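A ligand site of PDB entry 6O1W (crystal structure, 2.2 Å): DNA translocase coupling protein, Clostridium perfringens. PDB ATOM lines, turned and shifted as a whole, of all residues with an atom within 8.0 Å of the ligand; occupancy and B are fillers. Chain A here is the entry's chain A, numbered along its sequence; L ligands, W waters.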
ATOM      1  N   PHE A  34      14.799 -11.391  32.338  1.00  0.00           N
ATOM      2  CA  PHE A  34      15.794 -12.316  32.832  1.00  0.00           C
ATOM      3  C   PHE A  34      15.110 -13.697  32.766  1.00  0.00           C
ATOM      4  O   PHE A  34      14.182 -13.947  33.547  1.00  0.00           O
ATOM      5  CB  PHE A  34      16.175 -11.945  34.275  1.00  0.00           C
ATOM      6  CG  PHE A  34      17.336 -12.749  34.821  1.00  0.00           C
ATOM      7  CD1 PHE A  34      17.154 -14.045  35.286  1.00  0.00           C
ATOM      8  CD2 PHE A  34      18.617 -12.218  34.833  1.00  0.00           C
ATOM      9  CE1 PHE A  34      18.240 -14.804  35.747  1.00  0.00           C
ATOM     10  CE2 PHE A  34      19.703 -12.967  35.285  1.00  0.00           C
ATOM     11  CZ  PHE A  34      19.497 -14.253  35.769  1.00  0.00           C
ATOM     12  N   ILE A  35      15.517 -14.549  31.797  1.00  0.00           N
ATOM     13  CA  ILE A  35      14.965 -15.899  31.579  1.00  0.00           C
ATOM     14  C   ILE A  35      16.051 -16.932  31.890  1.00  0.00           C
ATOM     15  O   ILE A  35      17.029 -17.042  31.164  1.00  0.00           O
ATOM     16  CB  ILE A  35      14.380 -16.078  30.121  1.00  0.00           C
ATOM     17  CG1 ILE A  35      13.265 -15.044  29.831  1.00  0.00           C
ATOM     18  CG2 ILE A  35      13.859 -17.524  29.905  1.00  0.00           C
ATOM     19  CD1 ILE A  35      12.763 -14.984  28.365  1.00  0.00           C
ATOM     20  N   GLU A  36      15.884 -17.644  32.995  1.00  0.00           N
ATOM     21  CA  GLU A  36      16.806 -18.672  33.464  1.00  0.00           C
ATOM     22  C   GLU A  36      16.408 -20.051  32.912  1.00  0.00           C
ATOM     23  O   GLU A  36      15.223 -20.376  32.899  1.00  0.00           O
ATOM     24  CB  GLU A  36      16.799 -18.676  35.012  1.00  0.00           C
ATOM     25  CG  GLU A  36      16.991 -20.041  35.666  1.00  0.00           C
ATOM     26  CD  GLU A  36      18.199 -20.267  36.563  1.00  0.00           C
ATOM     27  OE1 GLU A  36      17.992 -20.659  37.732  1.00  0.00           O
ATOM     28  OE2 GLU A  36      19.355 -20.092  36.087  1.00  0.00           O
ATOM     29  N   ASP A  37      17.370 -20.867  32.474  1.00  0.00           N
ATOM     30  CA  ASP A  37      17.070 -22.266  32.073  1.00  0.00           C
ATOM     31  C   ASP A  37      17.498 -23.086  33.286  1.00  0.00           C
ATOM     32  O   ASP A  37      18.673 -23.102  33.618  1.00  0.00           O
ATOM     33  CB  ASP A  37      17.803 -22.724  30.797  1.00  0.00           C
ATOM     34  CG  ASP A  37      17.428 -24.118  30.300  1.00  0.00           C
ATOM     35  OD1 ASP A  37      17.364 -25.055  31.142  1.00  0.00           O
ATOM     36  OD2 ASP A  37      17.204 -24.283  29.077  1.00  0.00           O
ATOM     37  N   LYS A  38      16.535 -23.651  34.008  1.00  0.00           N
ATOM     38  CA  LYS A  38      16.748 -24.384  35.262  1.00  0.00           C
ATOM     39  C   LYS A  38      17.626 -25.637  35.145  1.00  0.00           C
ATOM     40  O   LYS A  38      18.344 -25.939  36.098  1.00  0.00           O
ATOM     41  CB  LYS A  38      15.385 -24.737  35.889  1.00  0.00           C
ATOM     42  CG  LYS A  38      15.373 -24.830  37.415  1.00  0.00           C
ATOM     43  CD  LYS A  38      14.138 -25.618  37.870  1.00  0.00           C
ATOM     44  CE  LYS A  38      13.841 -25.509  39.342  1.00  0.00           C
ATOM     45  NZ  LYS A  38      12.571 -26.196  39.697  1.00  0.00           N
ATOM     46  N   GLY A  39      17.571 -26.335  34.023  1.00  0.00           N
ATOM     47  CA  GLY A  39      18.397 -27.526  33.809  1.00  0.00           C
ATOM     48  C   GLY A  39      19.823 -27.205  33.381  1.00  0.00           C
ATOM     49  O   GLY A  39      20.772 -27.740  33.951  1.00  0.00           O
ATOM     50  N   THR A  40      19.987 -26.313  32.390  1.00  0.00           N
ATOM     51  CA  THR A  40      21.320 -25.934  31.880  1.00  0.00           C
ATOM     52  C   THR A  40      22.020 -24.868  32.698  1.00  0.00           C
ATOM     53  O   THR A  40      23.231 -24.739  32.600  1.00  0.00           O
ATOM     54  CB  THR A  40      21.263 -25.518  30.402  1.00  0.00           C
ATOM     55  OG1 THR A  40      20.623 -24.236  30.303  1.00  0.00           O
ATOM     56  CG2 THR A  40      20.540 -26.535  29.514  1.00  0.00           C
ATOM     57  N   ARG A  41      21.246 -24.067  33.463  1.00  0.00           N
ATOM     58  CA  ARG A  41      21.714 -22.937  34.277  1.00  0.00           C
ATOM     59  C   ARG A  41      22.289 -21.801  33.383  1.00  0.00           C
ATOM     60  O   ARG A  41      23.135 -21.021  33.815  1.00  0.00           O
ATOM     61  CB  ARG A  41      22.675 -23.381  35.408  1.00  0.00           C
ATOM     62  CG  ARG A  41      21.991 -24.297  36.427  1.00  0.00           C
ATOM     63  CD  ARG A  41      21.797 -23.629  37.773  1.00  0.00           C
ATOM     64  NE  ARG A  41      22.416 -24.407  38.845  1.00  0.00           N
ATOM     65  CZ  ARG A  41      23.221 -23.910  39.787  1.00  0.00           C
ATOM     66  NH1 ARG A  41      23.509 -22.610  39.804  1.00  0.00           N
ATOM     67  NH2 ARG A  41      23.744 -24.706  40.710  1.00  0.00           N
ATOM     68  N   ILE A  42      21.779 -21.714  32.158  1.00  0.00           N
ATOM     69  CA  ILE A  42      22.154 -20.661  31.210  1.00  0.00           C
ATOM     70  C   ILE A  42      20.980 -19.685  31.225  1.00  0.00           C
ATOM     71  O   ILE A  42      19.832 -20.118  31.081  1.00  0.00           O
ATOM     72  CB  ILE A  42      22.405 -21.205  29.768  1.00  0.00           C
ATOM     73  CG1 ILE A  42      23.562 -22.222  29.741  1.00  0.00           C
ATOM     74  CG2 ILE A  42      22.669 -20.046  28.777  1.00  0.00           C
ATOM     75  CD1 ILE A  42      23.552 -23.161  28.432  1.00  0.00           C
ATOM     76  N   ASP A  43      21.289 -18.385  31.403  1.00  0.00           N
ATOM     77  CA  ASP A  43      20.344 -17.269  31.481  1.00  0.00           C
ATOM     78  C   ASP A  43      20.343 -16.427  30.217  1.00  0.00           C
ATOM     79  O   ASP A  43      21.352 -16.305  29.556  1.00  0.00           O
ATOM     80  CB  ASP A  43      20.702 -16.353  32.683  1.00  0.00           C
ATOM     81  CG  ASP A  43      20.827 -17.066  34.018  1.00  0.00           C
ATOM     82  OD1 ASP A  43      19.832 -17.630  34.499  1.00  0.00           O
ATOM     83  OD2 ASP A  43      21.936 -17.063  34.592  1.00  0.00           O
ATOM     84  N   GLU A  44      19.211 -15.809  29.915  1.00  0.00           N
ATOM     85  CA  GLU A  44      19.029 -14.888  28.804  1.00  0.00           C
ATOM     86  C   GLU A  44      18.630 -13.557  29.454  1.00  0.00           C
ATOM     87  O   GLU A  44      17.560 -13.457  30.079  1.00  0.00           O
ATOM     88  CB  GLU A  44      17.959 -15.393  27.825  1.00  0.00           C
ATOM     89  CG  GLU A  44      17.825 -14.555  26.567  1.00  0.00           C
ATOM     90  CD  GLU A  44      16.506 -14.733  25.845  1.00  0.00           C
ATOM     91  OE1 GLU A  44      15.473 -14.238  26.349  1.00  0.00           O
ATOM     92  OE2 GLU A  44      16.501 -15.359  24.756  1.00  0.00           O
ATOM     93  N   ILE A  45      19.558 -12.585  29.423  1.00  0.00           N
ATOM     94  CA  ILE A  45      19.344 -11.273  30.021  1.00  0.00           C
ATOM     95  C   ILE A  45      19.184 -10.266  28.918  1.00  0.00           C
ATOM     96  O   ILE A  45      20.084 -10.111  28.079  1.00  0.00           O
ATOM     97  CB  ILE A  45      20.421 -10.859  31.060  1.00  0.00           C
ATOM     98  CG1 ILE A  45      20.915 -12.066  31.905  1.00  0.00           C
ATOM     99  CG2 ILE A  45      19.884  -9.745  31.953  1.00  0.00           C
ATOM    100  CD1 ILE A  45      22.314 -11.787  32.610  1.00  0.00           C
ATOM    101  N   THR A  46      18.032  -9.593  28.886  1.00  0.00           N
ATOM    102  CA  THR A  46      17.727  -8.615  27.854  1.00  0.00           C
ATOM    103  C   THR A  46      17.755  -7.239  28.447  1.00  0.00           C
ATOM    104  O   THR A  46      17.061  -6.969  29.427  1.00  0.00           O
ATOM    105  CB  THR A  46      16.386  -8.964  27.189  1.00  0.00           C
ATOM    106  OG1 THR A  46      16.420 -10.326  26.784  1.00  0.00           O
ATOM    107  CG2 THR A  46      16.067  -8.076  26.005  1.00  0.00           C
ATOM    108  N   GLU A  75      24.386 -10.435  21.874  1.00  0.00           N
ATOM    109  CA  GLU A  75      23.823 -10.199  20.538  1.00  0.00           C
ATOM    110  C   GLU A  75      22.854  -9.026  20.521  1.00  0.00           C
ATOM    111  O   GLU A  75      22.183  -8.755  21.524  1.00  0.00           O
ATOM    112  CB  GLU A  75      23.187 -11.481  19.944  1.00  0.00           C
ATOM    113  CG  GLU A  75      21.883 -11.921  20.594  1.00  0.00           C
ATOM    114  CD  GLU A  75      21.247 -13.184  20.031  1.00  0.00           C
ATOM    115  OE1 GLU A  75      21.412 -14.265  20.643  1.00  0.00           O
ATOM    116  OE2 GLU A  75      20.562 -13.090  18.985  1.00  0.00           O
ATOM    117  N   ILE A  84      21.018  -8.732  24.057  1.00  0.00           N
ATOM    118  CA  ILE A  84      20.649 -10.018  24.634  1.00  0.00           C
ATOM    119  C   ILE A  84      21.949 -10.682  25.030  1.00  0.00           C
ATOM    120  O   ILE A  84      22.814 -10.894  24.168  1.00  0.00           O
ATOM    121  CB  ILE A  84      19.862 -10.883  23.618  1.00  0.00           C
ATOM    122  CG1 ILE A  84      18.551 -10.174  23.167  1.00  0.00           C
ATOM    123  CG2 ILE A  84      19.605 -12.298  24.193  1.00  0.00           C
ATOM    124  CD1 ILE A  84      17.784 -10.804  21.997  1.00  0.00           C
ATOM    125  N   ILE A  85      22.098 -10.998  26.315  1.00  0.00           N
ATOM    126  CA  ILE A  85      23.291 -11.629  26.847  1.00  0.00           C
ATOM    127  C   ILE A  85      22.926 -13.051  27.233  1.00  0.00           C
ATOM    128  O   ILE A  85      21.913 -13.266  27.910  1.00  0.00           O
ATOM    129  CB  ILE A  85      23.813 -10.845  28.085  1.00  0.00           C
ATOM    130  CG1 ILE A  85      24.054  -9.342  27.772  1.00  0.00           C
ATOM    131  CG2 ILE A  85      25.081 -11.507  28.706  1.00  0.00           C
ATOM    132  CD1 ILE A  85      24.286  -8.470  28.991  1.00  0.00           C
ATOM    133  N   LYS A  86      23.752 -14.036  26.785  1.00  0.00           N
ATOM    134  CA  LYS A  86      23.629 -15.425  27.194  1.00  0.00           C
ATOM    135  C   LYS A  86      24.731 -15.594  28.220  1.00  0.00           C
ATOM    136  O   LYS A  86      25.895 -15.259  27.960  1.00  0.00           O
ATOM    137  CB  LYS A  86      23.786 -16.382  25.987  1.00  0.00           C
ATOM    138  CG  LYS A  86      22.673 -16.270  24.901  1.00  0.00           C
ATOM    139  CD  LYS A  86      21.203 -16.327  25.409  1.00  0.00           C
ATOM    140  CE  LYS A  86      20.826 -17.531  26.242  1.00  0.00           C
ATOM    141  NZ  LYS A  86      21.097 -18.807  25.547  1.00  0.00           N
ATOM    142  N   SER A  87      24.368 -15.974  29.443  1.00  0.00           N
ATOM    143  CA  SER A  87      25.371 -16.086  30.519  1.00  0.00           C
ATOM    144  C   SER A  87      25.083 -17.191  31.504  1.00  0.00           C
ATOM    145  O   SER A  87      23.999 -17.750  31.494  1.00  0.00           O
ATOM    146  CB  SER A  87      25.496 -14.762  31.280  1.00  0.00           C
ATOM    147  OG  SER A  87      24.250 -14.387  31.855  1.00  0.00           O
ATOM    148  N   SER A 305      19.564 -25.463  15.121  1.00  0.00           N
ATOM    149  CA  SER A 305      18.367 -25.798  15.899  1.00  0.00           C
ATOM    150  C   SER A 305      17.782 -27.177  15.570  1.00  0.00           C
ATOM    151  O   SER A 305      17.345 -27.868  16.484  1.00  0.00           O
ATOM    152  CB  SER A 305      17.286 -24.736  15.718  1.00  0.00           C
ATOM    153  OG  SER A 305      17.350 -23.767  16.743  1.00  0.00           O
ATOM    154  N   ASN A 314      14.364 -30.588  21.654  1.00  0.00           N
ATOM    155  CA  ASN A 314      14.439 -29.183  22.093  1.00  0.00           C
ATOM    156  C   ASN A 314      15.655 -28.561  21.367  1.00  0.00           C
ATOM    157  O   ASN A 314      16.427 -29.299  20.746  1.00  0.00           O
ATOM    158  CB  ASN A 314      14.482 -29.026  23.623  1.00  0.00           C
ATOM    159  CG  ASN A 314      15.724 -29.543  24.301  1.00  0.00           C
ATOM    160  OD1 ASN A 314      16.837 -29.213  23.925  1.00  0.00           O
ATOM    161  ND2 ASN A 314      15.553 -30.358  25.330  1.00  0.00           N
ATOM    162  N   THR A 315      15.844 -27.237  21.449  1.00  0.00           N
ATOM    163  CA  THR A 315      16.909 -26.528  20.742  1.00  0.00           C
ATOM    164  C   THR A 315      18.085 -26.123  21.668  1.00  0.00           C
ATOM    165  O   THR A 315      18.879 -25.271  21.272  1.00  0.00           O
ATOM    166  CB  THR A 315      16.302 -25.250  20.112  1.00  0.00           C
ATOM    167  OG1 THR A 315      15.905 -24.382  21.178  1.00  0.00           O
ATOM    168  CG2 THR A 315      15.101 -25.537  19.185  1.00  0.00           C
ATOM    169  N   LYS A 316      18.192 -26.708  22.861  1.00  0.00           N
ATOM    170  CA  LYS A 316      19.200 -26.305  23.858  1.00  0.00           C
ATOM    171  C   LYS A 316      20.662 -26.569  23.498  1.00  0.00           C
ATOM    172  O   LYS A 316      21.531 -25.938  24.100  1.00  0.00           O
ATOM    173  CB  LYS A 316      18.902 -26.905  25.240  1.00  0.00           C
ATOM    174  CG  LYS A 316      17.529 -26.522  25.782  1.00  0.00           C
ATOM    175  CD  LYS A 316      17.257 -27.295  27.098  1.00  0.00           C
ATOM    176  CE  LYS A 316      15.810 -27.307  27.500  1.00  0.00           C
ATOM    177  NZ  LYS A 316      15.327 -25.932  27.780  1.00  0.00           N
ATOM    178  N   ALA A 317      20.966 -27.493  22.547  1.00  0.00           N
ATOM    179  CA  ALA A 317      22.387 -27.728  22.186  1.00  0.00           C
ATOM    180  C   ALA A 317      23.022 -26.479  21.519  1.00  0.00           C
ATOM    181  O   ALA A 317      24.227 -26.317  21.537  1.00  0.00           O
ATOM    182  CB  ALA A 317      22.521 -28.957  21.288  1.00  0.00           C
ATOM    183  N   LYS A 318      22.194 -25.540  21.008  1.00  0.00           N
ATOM    184  CA  LYS A 318      22.701 -24.296  20.407  1.00  0.00           C
ATOM    185  C   LYS A 318      23.181 -23.274  21.475  1.00  0.00           C
ATOM    186  O   LYS A 318      23.852 -22.312  21.122  1.00  0.00           O
ATOM    187  CB  LYS A 318      21.639 -23.689  19.445  1.00  0.00           C
ATOM    188  CG  LYS A 318      20.599 -22.782  20.129  1.00  0.00           C
ATOM    189  CD  LYS A 318      19.241 -22.702  19.429  1.00  0.00           C
ATOM    190  CE  LYS A 318      18.235 -21.838  20.190  1.00  0.00           C
ATOM    191  NZ  LYS A 318      17.935 -22.323  21.578  1.00  0.00           N
ATOM    192  N   ASP A 319      22.791 -23.463  22.743  1.00  0.00           N
ATOM    193  CA  ASP A 319      23.075 -22.539  23.862  1.00  0.00           C
ATOM    194  C   ASP A 319      24.355 -22.867  24.603  1.00  0.00           C
ATOM    195  O   ASP A 319      24.787 -22.058  25.432  1.00  0.00           O
ATOM    196  CB  ASP A 319      21.941 -22.603  24.908  1.00  0.00           C
ATOM    197  CG  ASP A 319      20.529 -22.516  24.387  1.00  0.00           C
ATOM    198  OD1 ASP A 319      20.309 -21.827  23.393  1.00  0.00           O
ATOM    199  OD2 ASP A 319      19.631 -23.136  25.022  1.00  0.00           O
HETATM  200  C1  LIG L   1      17.192 -20.110  24.576  1.00  0.00           C
HETATM  201  C2  LIG L   1      16.426 -21.178  25.348  1.00  0.00           C
HETATM  202  C3  LIG L   1      16.717 -21.068  26.848  1.00  0.00           C
HETATM  203  C4  LIG L   1      16.497 -19.642  27.330  1.00  0.00           C
HETATM  204  C5  LIG L   1      16.915 -19.424  28.768  1.00  0.00           C
HETATM  205  C6  LIG L   1      16.959 -18.724  25.170  1.00  0.00           C
HETATM  206  O1  LIG L   1      17.767 -17.819  24.512  1.00  0.00           O
HETATM  207  O2  LIG L   1      16.799 -20.090  23.209  1.00  0.00           O
HETATM  208  O3  LIG L   1      16.800 -22.469  24.892  1.00  0.00           O
HETATM  209  O4  LIG L   1      15.909 -21.988  27.590  1.00  0.00           O
HETATM  210  O5  LIG L   1      17.294 -18.735  26.555  1.00  0.00           O
HETATM  211  O6  LIG L   1      18.324 -19.535  28.930  1.00  0.00           O
HETATM  212  O   HOH W   1      20.011 -20.892  27.011  1.00  0.00           O
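Ile 35 touches the ligand. Asp 43 touches the ligand (C to O6, 3.9 Å). Lys 86 touches the ligand (CE to O1, 3.5 Å). NZ of Lys 316 touches O4 of the ligand (3.99 Å). Hydrophobic or aromatic side chains within 4 Å of the ligand: Ile 35.
The backbone NH of Asp 37 lies within hydrogen-bond range of the backbone carbonyl oxygen of Ile 42 (2.9 Å). The side-chain amino group of Lys 318 is in hydrogen-bond range of the side-chain hydroxyl of Thr 315, 2.9 Å away. The backbone NH of Ile 42 lies close to the side-chain hydroxyl of Thr 40 (3.3 Å). The backbone NH (N) of Glu 44 sits at hydrogen-bond distance from the backbone carbonyl oxygen (O) of Ile 35, 2.8 Å away. The side-chain amino group (NZ) of Lys 318 lies within salt-bridge range of the side-chain carboxylate (OD1) of Asp 319, 3.0 Å away. The side-chain carboxylate (OD2) of Asp 37 lies within salt-bridge range of the side-chain amino group (NZ) of Lys 316, 2.8 Å away. The side-chain carboxylate (OD1) of Asp 37 sits at hydrogen-bond distance from the backbone NH (N) of Gly 39, 3.2 Å away. OD1 of Asp 319 lies within salt-bridge range of NZ of Lys 86.
The backbone carbonyl oxygen (O) of Ile 42 is in hydrogen-bond range of an oxygen (O6) of the ligand. An oxygen (O1) of the ligand is in hydrogen-bond range of the side-chain carboxylate (OE2) of Glu 44 (2.8 Å). O4 of the ligand is in hydrogen-bond range of OD2 of Asp 37 (3.0 Å). NZ of Lys 318 lies within hydrogen-bond range of O2 of the ligand, 3.0 Å away. The side-chain carboxylate (OD2) of Asp 319 is in hydrogen-bond range of an oxygen (O3) of the ligand (2.9 Å).
Water W1 lies within hydrogen-bond range of NZ of Lys 86 (2.8 Å), O6 of the ligand (2.9 Å) and OD2 of Asp 319 (3.0 Å).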
